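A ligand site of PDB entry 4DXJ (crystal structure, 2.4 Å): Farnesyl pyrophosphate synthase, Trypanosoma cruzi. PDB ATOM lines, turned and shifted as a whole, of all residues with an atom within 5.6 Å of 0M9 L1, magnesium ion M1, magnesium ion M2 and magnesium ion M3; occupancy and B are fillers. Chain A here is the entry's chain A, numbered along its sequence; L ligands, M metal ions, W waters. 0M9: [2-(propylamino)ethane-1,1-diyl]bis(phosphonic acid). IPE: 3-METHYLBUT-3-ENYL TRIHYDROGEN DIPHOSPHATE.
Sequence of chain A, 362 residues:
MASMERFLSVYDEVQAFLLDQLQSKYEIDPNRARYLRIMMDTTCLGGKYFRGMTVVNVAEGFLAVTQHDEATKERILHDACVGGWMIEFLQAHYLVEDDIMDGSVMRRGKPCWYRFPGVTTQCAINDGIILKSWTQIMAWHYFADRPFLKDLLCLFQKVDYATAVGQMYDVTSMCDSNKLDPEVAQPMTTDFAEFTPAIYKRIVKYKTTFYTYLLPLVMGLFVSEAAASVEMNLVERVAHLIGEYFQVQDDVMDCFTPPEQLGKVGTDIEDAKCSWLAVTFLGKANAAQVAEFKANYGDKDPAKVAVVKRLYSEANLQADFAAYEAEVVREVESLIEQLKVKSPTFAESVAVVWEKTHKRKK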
ATOM      1  N   TYR A  94      27.674   8.094  -9.521  1.00  0.00           N
ATOM      2  CA  TYR A  94      26.753   8.468  -8.447  1.00  0.00           C
ATOM      3  C   TYR A  94      25.716   9.500  -8.884  1.00  0.00           C
ATOM      4  O   TYR A  94      24.535   9.302  -8.629  1.00  0.00           O
ATOM      5  CB  TYR A  94      27.512   8.843  -7.133  1.00  0.00           C
ATOM      6  CG  TYR A  94      27.853   7.580  -6.385  1.00  0.00           C
ATOM      7  CD1 TYR A  94      29.163   7.195  -6.112  1.00  0.00           C
ATOM      8  CD2 TYR A  94      26.827   6.702  -6.014  1.00  0.00           C
ATOM      9  CE1 TYR A  94      29.436   5.968  -5.474  1.00  0.00           C
ATOM     10  CE2 TYR A  94      27.071   5.515  -5.387  1.00  0.00           C
ATOM     11  CZ  TYR A  94      28.362   5.136  -5.117  1.00  0.00           C
ATOM     12  OH  TYR A  94      28.509   3.910  -4.470  1.00  0.00           O
ATOM     13  N   LEU A  95      26.160  10.565  -9.576  1.00  0.00           N
ATOM     14  CA  LEU A  95      25.268  11.627 -10.017  1.00  0.00           C
ATOM     15  C   LEU A  95      24.213  11.127 -10.982  1.00  0.00           C
ATOM     16  O   LEU A  95      23.053  11.529 -10.901  1.00  0.00           O
ATOM     17  CB  LEU A  95      26.043  12.807 -10.609  1.00  0.00           C
ATOM     18  CG  LEU A  95      27.085  13.464  -9.693  1.00  0.00           C
ATOM     19  CD1 LEU A  95      27.716  14.692 -10.357  1.00  0.00           C
ATOM     20  CD2 LEU A  95      26.519  13.832  -8.284  1.00  0.00           C
ATOM     21  N   ASP A  98      21.812   9.092  -8.857  1.00  0.00           N
ATOM     22  CA  ASP A  98      21.255   9.997  -7.860  1.00  0.00           C
ATOM     23  C   ASP A  98      20.176  10.915  -8.428  1.00  0.00           C
ATOM     24  O   ASP A  98      19.153  11.187  -7.766  1.00  0.00           O
ATOM     25  CB  ASP A  98      22.356  10.812  -7.187  1.00  0.00           C
ATOM     26  CG  ASP A  98      21.816  11.791  -6.173  1.00  0.00           C
ATOM     27  OD1 ASP A  98      21.624  11.389  -5.006  1.00  0.00           O
ATOM     28  OD2 ASP A  98      21.582  12.977  -6.527  1.00  0.00           O
ATOM     29  N   ASP A  99      20.388  11.394  -9.659  1.00  0.00           N
ATOM     30  CA  ASP A  99      19.423  12.271 -10.296  1.00  0.00           C
ATOM     31  C   ASP A  99      18.122  11.550 -10.590  1.00  0.00           C
ATOM     32  O   ASP A  99      17.053  12.137 -10.437  1.00  0.00           O
ATOM     33  CB  ASP A  99      20.004  12.937 -11.556  1.00  0.00           C
ATOM     34  CG  ASP A  99      20.967  14.060 -11.220  1.00  0.00           C
ATOM     35  OD1 ASP A  99      20.851  14.633 -10.132  1.00  0.00           O
ATOM     36  OD2 ASP A  99      21.855  14.369 -12.036  1.00  0.00           O
ATOM     37  N   ASP A 102      16.498  10.952  -7.106  1.00  0.00           N
ATOM     38  CA  ASP A 102      15.960  12.168  -6.514  1.00  0.00           C
ATOM     39  C   ASP A 102      14.948  12.865  -7.429  1.00  0.00           C
ATOM     40  O   ASP A 102      14.423  13.914  -7.076  1.00  0.00           O
ATOM     41  CB  ASP A 102      17.086  13.117  -6.106  1.00  0.00           C
ATOM     42  CG  ASP A 102      18.024  12.525  -5.066  1.00  0.00           C
ATOM     43  OD1 ASP A 102      17.718  11.426  -4.525  1.00  0.00           O
ATOM     44  OD2 ASP A 102      19.077  13.146  -4.766  1.00  0.00           O
ATOM     45  N   SER A 104      15.444  14.529 -10.212  1.00  0.00           N
ATOM     46  CA  SER A 104      15.960  15.846 -10.584  1.00  0.00           C
ATOM     47  C   SER A 104      15.837  16.131 -12.088  1.00  0.00           C
ATOM     48  O   SER A 104      15.637  15.206 -12.888  1.00  0.00           O
ATOM     49  CB  SER A 104      17.429  15.985 -10.159  1.00  0.00           C
ATOM     50  OG  SER A 104      17.568  15.977  -8.747  1.00  0.00           O
ATOM     51  N   ARG A 107      21.430  19.100 -14.212  1.00  0.00           N
ATOM     52  CA  ARG A 107      22.732  18.859 -13.630  1.00  0.00           C
ATOM     53  C   ARG A 107      23.773  19.548 -14.501  1.00  0.00           C
ATOM     54  O   ARG A 107      23.817  19.336 -15.714  1.00  0.00           O
ATOM     55  CB  ARG A 107      23.000  17.346 -13.531  1.00  0.00           C
ATOM     56  CG  ARG A 107      24.452  16.970 -13.216  1.00  0.00           C
ATOM     57  CD  ARG A 107      24.764  17.138 -11.738  1.00  0.00           C
ATOM     58  NE  ARG A 107      23.933  16.267 -10.914  1.00  0.00           N
ATOM     59  CZ  ARG A 107      23.912  16.283  -9.585  1.00  0.00           C
ATOM     60  NH1 ARG A 107      24.693  17.125  -8.894  1.00  0.00           N
ATOM     61  NH2 ARG A 107      23.108  15.450  -8.940  1.00  0.00           N
ATOM     62  N   THR A 163      29.671   4.811   0.344  1.00  0.00           N
ATOM     63  CA  THR A 163      28.810   5.738  -0.398  1.00  0.00           C
ATOM     64  C   THR A 163      27.459   5.100  -0.771  1.00  0.00           C
ATOM     65  O   THR A 163      26.413   5.763  -0.704  1.00  0.00           O
ATOM     66  CB  THR A 163      29.527   6.243  -1.673  1.00  0.00           C
ATOM     67  OG1 THR A 163      30.834   6.703  -1.330  1.00  0.00           O
ATOM     68  CG2 THR A 163      28.727   7.371  -2.329  1.00  0.00           C
ATOM     69  N   GLN A 167      23.919   6.457   0.538  1.00  0.00           N
ATOM     70  CA  GLN A 167      22.821   6.766  -0.363  1.00  0.00           C
ATOM     71  C   GLN A 167      21.534   6.112   0.124  1.00  0.00           C
ATOM     72  O   GLN A 167      20.442   6.680  -0.019  1.00  0.00           O
ATOM     73  CB  GLN A 167      23.151   6.327  -1.793  1.00  0.00           C
ATOM     74  CG  GLN A 167      24.085   7.286  -2.583  1.00  0.00           C
ATOM     75  CD  GLN A 167      23.508   8.701  -2.756  1.00  0.00           C
ATOM     76  OE1 GLN A 167      23.457   9.478  -1.800  1.00  0.00           O
ATOM     77  NE2 GLN A 167      23.088   9.023  -3.964  1.00  0.00           N
ATOM     78  N   ASP A 170      20.397   8.203   2.897  1.00  0.00           N
ATOM     79  CA  ASP A 170      19.830   9.427   2.328  1.00  0.00           C
ATOM     80  C   ASP A 170      18.441   9.196   1.759  1.00  0.00           C
ATOM     81  O   ASP A 170      17.515   9.931   2.061  1.00  0.00           O
ATOM     82  CB  ASP A 170      20.735  10.044   1.255  1.00  0.00           C
ATOM     83  CG  ASP A 170      20.086  11.248   0.571  1.00  0.00           C
ATOM     84  OD1 ASP A 170      20.482  12.389   0.882  1.00  0.00           O
ATOM     85  OD2 ASP A 170      19.163  11.050  -0.250  1.00  0.00           O
ATOM     86  N   LYS A 207      27.318   9.149   2.572  1.00  0.00           N
ATOM     87  CA  LYS A 207      26.954   9.464   1.186  1.00  0.00           C
ATOM     88  C   LYS A 207      27.991  10.359   0.500  1.00  0.00           C
ATOM     89  O   LYS A 207      28.153  10.268  -0.721  1.00  0.00           O
ATOM     90  CB  LYS A 207      25.527  10.039   1.059  1.00  0.00           C
ATOM     91  CG  LYS A 207      25.399  11.534   1.244  1.00  0.00           C
ATOM     92  CD  LYS A 207      23.967  12.012   0.976  1.00  0.00           C
ATOM     93  CE  LYS A 207      23.796  13.488   1.341  1.00  0.00           C
ATOM     94  NZ  LYS A 207      22.530  14.118   0.800  1.00  0.00           N
ATOM     95  N   THR A 208      28.719  11.169   1.274  1.00  0.00           N
ATOM     96  CA  THR A 208      29.515  12.246   0.703  1.00  0.00           C
ATOM     97  C   THR A 208      31.006  12.267   1.056  1.00  0.00           C
ATOM     98  O   THR A 208      31.852  12.332   0.154  1.00  0.00           O
ATOM     99  CB  THR A 208      28.894  13.626   1.036  1.00  0.00           C
ATOM    100  OG1 THR A 208      27.617  13.730   0.392  1.00  0.00           O
ATOM    101  CG2 THR A 208      29.796  14.764   0.559  1.00  0.00           C
ATOM    102  N   TYR A 211      33.989   9.581  -0.464  1.00  0.00           N
ATOM    103  CA  TYR A 211      34.409   9.688  -1.856  1.00  0.00           C
ATOM    104  C   TYR A 211      34.767  11.126  -2.284  1.00  0.00           C
ATOM    105  O   TYR A 211      35.496  11.300  -3.256  1.00  0.00           O
ATOM    106  CB  TYR A 211      33.372   9.076  -2.796  1.00  0.00           C
ATOM    107  CG  TYR A 211      32.314  10.034  -3.296  1.00  0.00           C
ATOM    108  CD1 TYR A 211      32.508  10.755  -4.464  1.00  0.00           C
ATOM    109  CD2 TYR A 211      31.121  10.187  -2.616  1.00  0.00           C
ATOM    110  CE1 TYR A 211      31.538  11.630  -4.929  1.00  0.00           C
ATOM    111  CE2 TYR A 211      30.141  11.064  -3.083  1.00  0.00           C
ATOM    112  CZ  TYR A 211      30.361  11.774  -4.233  1.00  0.00           C
ATOM    113  OH  TYR A 211      29.397  12.638  -4.693  1.00  0.00           O
ATOM    114  N   GLN A 247      28.649  19.229   2.241  1.00  0.00           N
ATOM    115  CA  GLN A 247      27.253  18.818   2.087  1.00  0.00           C
ATOM    116  C   GLN A 247      26.256  19.806   2.683  1.00  0.00           C
ATOM    117  O   GLN A 247      25.159  19.983   2.160  1.00  0.00           O
ATOM    118  CB  GLN A 247      27.059  17.440   2.710  1.00  0.00           C
ATOM    119  CG  GLN A 247      25.741  16.769   2.344  1.00  0.00           C
ATOM    120  CD  GLN A 247      25.562  16.611   0.839  1.00  0.00           C
ATOM    121  OE1 GLN A 247      26.434  16.082   0.154  1.00  0.00           O
ATOM    122  NE2 GLN A 247      24.414  17.043   0.337  1.00  0.00           N
ATOM    123  N   ASP A 250      25.993  22.326   0.139  1.00  0.00           N
ATOM    124  CA  ASP A 250      25.151  21.754  -0.911  1.00  0.00           C
ATOM    125  C   ASP A 250      23.645  21.830  -0.578  1.00  0.00           C
ATOM    126  O   ASP A 250      22.837  22.181  -1.454  1.00  0.00           O
ATOM    127  CB  ASP A 250      25.541  20.298  -1.160  1.00  0.00           C
ATOM    128  CG  ASP A 250      24.768  19.691  -2.316  1.00  0.00           C
ATOM    129  OD1 ASP A 250      25.086  20.008  -3.493  1.00  0.00           O
ATOM    130  OD2 ASP A 250      23.828  18.915  -2.055  1.00  0.00           O
ATOM    131  N   ASP A 251      23.307  21.473   0.666  1.00  0.00           N
ATOM    132  CA  ASP A 251      21.935  21.529   1.180  1.00  0.00           C
ATOM    133  C   ASP A 251      21.391  22.946   1.211  1.00  0.00           C
ATOM    134  O   ASP A 251      20.239  23.189   0.821  1.00  0.00           O
ATOM    135  CB  ASP A 251      21.887  20.951   2.602  1.00  0.00           C
ATOM    136  CG  ASP A 251      22.032  19.448   2.637  1.00  0.00           C
ATOM    137  OD1 ASP A 251      22.219  18.805   1.576  1.00  0.00           O
ATOM    138  OD2 ASP A 251      21.944  18.897   3.748  1.00  0.00           O
ATOM    139  N   ASP A 254      20.935  24.165  -2.431  1.00  0.00           N
ATOM    140  CA  ASP A 254      19.765  23.500  -3.003  1.00  0.00           C
ATOM    141  C   ASP A 254      18.512  24.359  -2.883  1.00  0.00           C
ATOM    142  O   ASP A 254      17.655  24.333  -3.762  1.00  0.00           O
ATOM    143  CB  ASP A 254      19.500  22.178  -2.296  1.00  0.00           C
ATOM    144  CG  ASP A 254      18.460  21.333  -3.009  1.00  0.00           C
ATOM    145  OD1 ASP A 254      18.825  20.656  -3.994  1.00  0.00           O
ATOM    146  OD2 ASP A 254      17.278  21.341  -2.592  1.00  0.00           O
ATOM    147  N   LYS A 264      22.011  23.230 -11.133  1.00  0.00           N
ATOM    148  CA  LYS A 264      21.010  22.192 -10.869  1.00  0.00           C
ATOM    149  C   LYS A 264      19.746  22.807 -10.279  1.00  0.00           C
ATOM    150  O   LYS A 264      19.766  23.950  -9.836  1.00  0.00           O
ATOM    151  CB  LYS A 264      21.592  21.082  -9.986  1.00  0.00           C
ATOM    152  CG  LYS A 264      22.396  21.555  -8.792  1.00  0.00           C
ATOM    153  CD  LYS A 264      23.108  20.377  -8.132  1.00  0.00           C
ATOM    154  CE  LYS A 264      23.429  20.681  -6.681  1.00  0.00           C
ATOM    155  NZ  LYS A 264      24.343  19.665  -6.095  1.00  0.00           N
ATOM    156  N   THR A 267      15.602  19.892  -5.210  1.00  0.00           N
ATOM    157  CA  THR A 267      14.553  18.894  -4.968  1.00  0.00           C
ATOM    158  C   THR A 267      14.474  18.460  -3.499  1.00  0.00           C
ATOM    159  O   THR A 267      13.672  17.577  -3.168  1.00  0.00           O
ATOM    160  CB  THR A 267      14.731  17.593  -5.824  1.00  0.00           C
ATOM    161  OG1 THR A 267      16.041  17.027  -5.600  1.00  0.00           O
ATOM    162  CG2 THR A 267      14.517  17.866  -7.299  1.00  0.00           C
ATOM    163  N   ASP A 268      15.276  19.056  -2.632  1.00  0.00           N
ATOM    164  CA  ASP A 268      15.361  18.604  -1.243  1.00  0.00           C
ATOM    165  C   ASP A 268      14.043  18.726  -0.480  1.00  0.00           C
ATOM    166  O   ASP A 268      13.633  17.786   0.202  1.00  0.00           O
ATOM    167  CB  ASP A 268      16.516  19.284  -0.475  1.00  0.00           C
ATOM    168  CG  ASP A 268      17.876  18.673  -0.794  1.00  0.00           C
ATOM    169  OD1 ASP A 268      17.945  17.616  -1.464  1.00  0.00           O
ATOM    170  OD2 ASP A 268      18.902  19.256  -0.383  1.00  0.00           O
ATOM    171  N   LYS A 273      13.747  15.416   2.063  1.00  0.00           N
ATOM    172  CA  LYS A 273      15.095  15.050   2.463  1.00  0.00           C
ATOM    173  C   LYS A 273      15.456  15.547   3.856  1.00  0.00           C
ATOM    174  O   LYS A 273      15.085  16.647   4.251  1.00  0.00           O
ATOM    175  CB  LYS A 273      16.123  15.570   1.444  1.00  0.00           C
ATOM    176  CG  LYS A 273      16.128  14.835   0.114  1.00  0.00           C
ATOM    177  CD  LYS A 273      16.739  13.443   0.241  1.00  0.00           C
ATOM    178  CE  LYS A 273      16.203  12.491  -0.808  1.00  0.00           C
ATOM    179  NZ  LYS A 273      16.590  12.885  -2.173  1.00  0.00           N
HETATM  180  O1  0M9 L   1      24.354  17.053  -6.181  1.00  0.00           O
HETATM  181  P1  0M9 L   1      23.078  16.676  -5.479  1.00  0.00           P
HETATM  182  O3  0M9 L   1      22.590  17.738  -4.521  1.00  0.00           O
HETATM  183  O2  0M9 L   1      22.013  16.192  -6.420  1.00  0.00           O
HETATM  184  C9  0M9 L   1      23.388  15.131  -4.547  1.00  0.00           C
HETATM  185  P2  0M9 L   1      22.423  14.992  -2.994  1.00  0.00           P
HETATM  186  O4  0M9 L   1      23.200  14.090  -2.061  1.00  0.00           O
HETATM  187  O5  0M9 L   1      22.217  16.396  -2.454  1.00  0.00           O
HETATM  188  O6  0M9 L   1      21.196  14.319  -3.551  1.00  0.00           O
HETATM  189  C8  0M9 L   1      24.813  14.730  -4.161  1.00  0.00           C
HETATM  190  N1  0M9 L   1      24.817  13.279  -4.144  1.00  0.00           N
HETATM  191  C7  0M9 L   1      26.061  12.568  -4.013  1.00  0.00           C
HETATM  192  C6  0M9 L   1      25.797  11.073  -4.099  1.00  0.00           C
HETATM  193  C5  0M9 L   1      26.613  10.383  -3.053  1.00  0.00           C
HETATM  194  C1  IPE L   2      27.635  17.359  -5.808  1.00  0.00           C
HETATM  195  O1  IPE L   2      29.033  17.349  -6.063  1.00  0.00           O
HETATM  196  C2  IPE L   2      27.262  16.066  -5.095  1.00  0.00           C
HETATM  197  C3  IPE L   2      27.790  16.037  -3.668  1.00  0.00           C
HETATM  198  C4  IPE L   2      28.645  15.095  -3.315  1.00  0.00           C
HETATM  199  C5  IPE L   2      27.329  17.036  -2.653  1.00  0.00           C
HETATM  200  PA  IPE L   2      29.761  18.592  -6.791  1.00  0.00           P
HETATM  201  O1A IPE L   2      31.185  18.632  -6.313  1.00  0.00           O
HETATM  202  O2A IPE L   2      28.833  19.785  -6.633  1.00  0.00           O
HETATM  203  O3A IPE L   2      29.700  18.105  -8.346  1.00  0.00           O
HETATM  204  PB  IPE L   2      30.714  18.506  -9.552  1.00  0.00           P
HETATM  205  O1B IPE L   2      31.760  19.474  -9.006  1.00  0.00           O
HETATM  206  O2B IPE L   2      31.292  17.179  -9.993  1.00  0.00           O
HETATM  207  O3B IPE L   2      29.727  19.057 -10.547  1.00  0.00           O
HETATM  208 MG    MG M   1      20.748  12.458  -3.487  1.00  0.00          MG
HETATM  209 MG    MG M   2      20.681  14.669  -5.660  1.00  0.00          MG
HETATM  210 MG    MG M   3      21.978  18.357  -2.917  1.00  0.00          MG
HETATM  211  O   HOH W   1      19.979  18.101  -3.443  1.00  0.00           O
HETATM  212  O   HOH W   2      22.070  11.747  -1.949  1.00  0.00           O
HETATM  213  O   HOH W   3      21.447  18.942  -1.011  1.00  0.00           O
HETATM  214  O   HOH W   4      19.585  10.519  -3.127  1.00  0.00           O
HETATM  215  O   HOH W   5      19.744  14.738  -7.838  1.00  0.00           O
HETATM  216  O   HOH W   6      19.317  15.972  -4.781  1.00  0.00           O
HETATM  217  O   HOH W   7      20.729  18.096  -7.610  1.00  0.00           O
HETATM  218  O   HOH W   8      19.482  13.049  -1.965  1.00  0.00           O
HETATM  219  O   HOH W   9      22.016  20.194  -3.629  1.00  0.00           O
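Water W4 lies within hydrogen-bond range of OD1 of Asp 102 and OD2 of Asp 170. Water W2 lies within hydrogen-bond range of O4 of 0M9 L1, OE1 of Gln 167 and OD1 of Asp 170. Water W8 bridges OD2 of Asp 170 (2.7 Å) and NZ of Lys 273 (2.9 Å). Water W1 lies within hydrogen-bond range of OD1 of Asp 254 (2.9 Å) and OD1 of Asp 268 (2.9 Å). Water W3 lies within hydrogen-bond range of OD2 of Asp 268 (2.6 Å) and OD1 of Asp 251 (2.7 Å). Water W9 lies within hydrogen-bond range of O of Asp 250, OD1 of Asp 254 and NZ of Lys 264.
NZ of Lys 273 is in salt-bridge range of OD2 of Asp 170 (3.7 Å). NH2 of Arg 107 lies within salt-bridge range of OD1 of Asp 99. NZ of Lys 264 is in salt-bridge range of OD1 of Asp 250 (2.7 Å). The side-chain amide nitrogen of Gln 247 lies within hydrogen-bond range of the side-chain carboxylate of Asp 251, 3.1 Å away. The side-chain amino group (NZ) of Lys 207 is in salt-bridge range of the side-chain carboxylate (OD1) of Asp 170 (2.7 Å). NE2 of Gln 247 lies close to OD2 of Asp 250 (3.1 Å). The side-chain hydroxyl (OG1) of Thr 208 lies within hydrogen-bond range of the side-chain amide oxygen (OE1) of Gln 247, at 2.6 Å. OD2 of Asp 98 sits close to NH2 of Arg 107.
OD2 of Asp 170 touches magnesium ion M1, 3.9 Å away. Of the 21 residues printed, 3 come within 4 Å of magnesium ion M1. The nearest printed residue that does not touch magnesium ion M1 is Gln 167 (4.2 Å).
Two residues have an atom within 4 Å of magnesium ion M2: Asp 98 and Asp 102. Along chain A the residues within 4 Å of magnesium ion M2 span positions 98 to 102.
Magnesium ion M1 is bound by an oxygen (O6) of 0M9 L1 (1.9 Å), the side-chain carboxylate of Asp 98 (2.1 Å), water W8 (2.1 Å), water W2 (2.1 Å), the side-chain carboxylate of Asp 102 (2.2 Å) and water W4 (2.3 Å).
Magnesium ion M3 is bound by O3 of 0M9 L1 (1.8 Å), water W9 (2.0 Å), O5 of 0M9 L1 (2.0 Å), water W3 (2.1 Å), water W1 (2.1 Å) and OD2 of Asp 250 (2.1 Å).
An oxygen (O4) of 0M9 L1 is in salt-bridge range of the side-chain amino group (NZ) of Lys 207. The guanidinium group of Arg 107 is in salt-bridge range of an oxygen (O1) of 0M9 L1, 2.7 Å away. The side-chain amino group of Lys 264 is in salt-bridge range of an oxygen (O1) of 0M9 L1.
One residue has an atom within 4 Å of magnesium ion M3: Asp 250.
Thr 163 touches 0M9 L1 (CG2 to C5, 3.8 Å). Gln 167 touches 0M9 L1. Tyr 211 touches 0M9 L1. Gln 247 touches 0M9 L1 (NE2 to O5, 3.6 Å).
Magnesium ion M2 is bound by water W6, the side-chain carboxylate (OD2) of Asp 98, an oxygen (O2) of 0M9 L1, an oxygen (O6) of 0M9 L1, water W5 and the side-chain carboxylate (OD2) of Asp 102.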
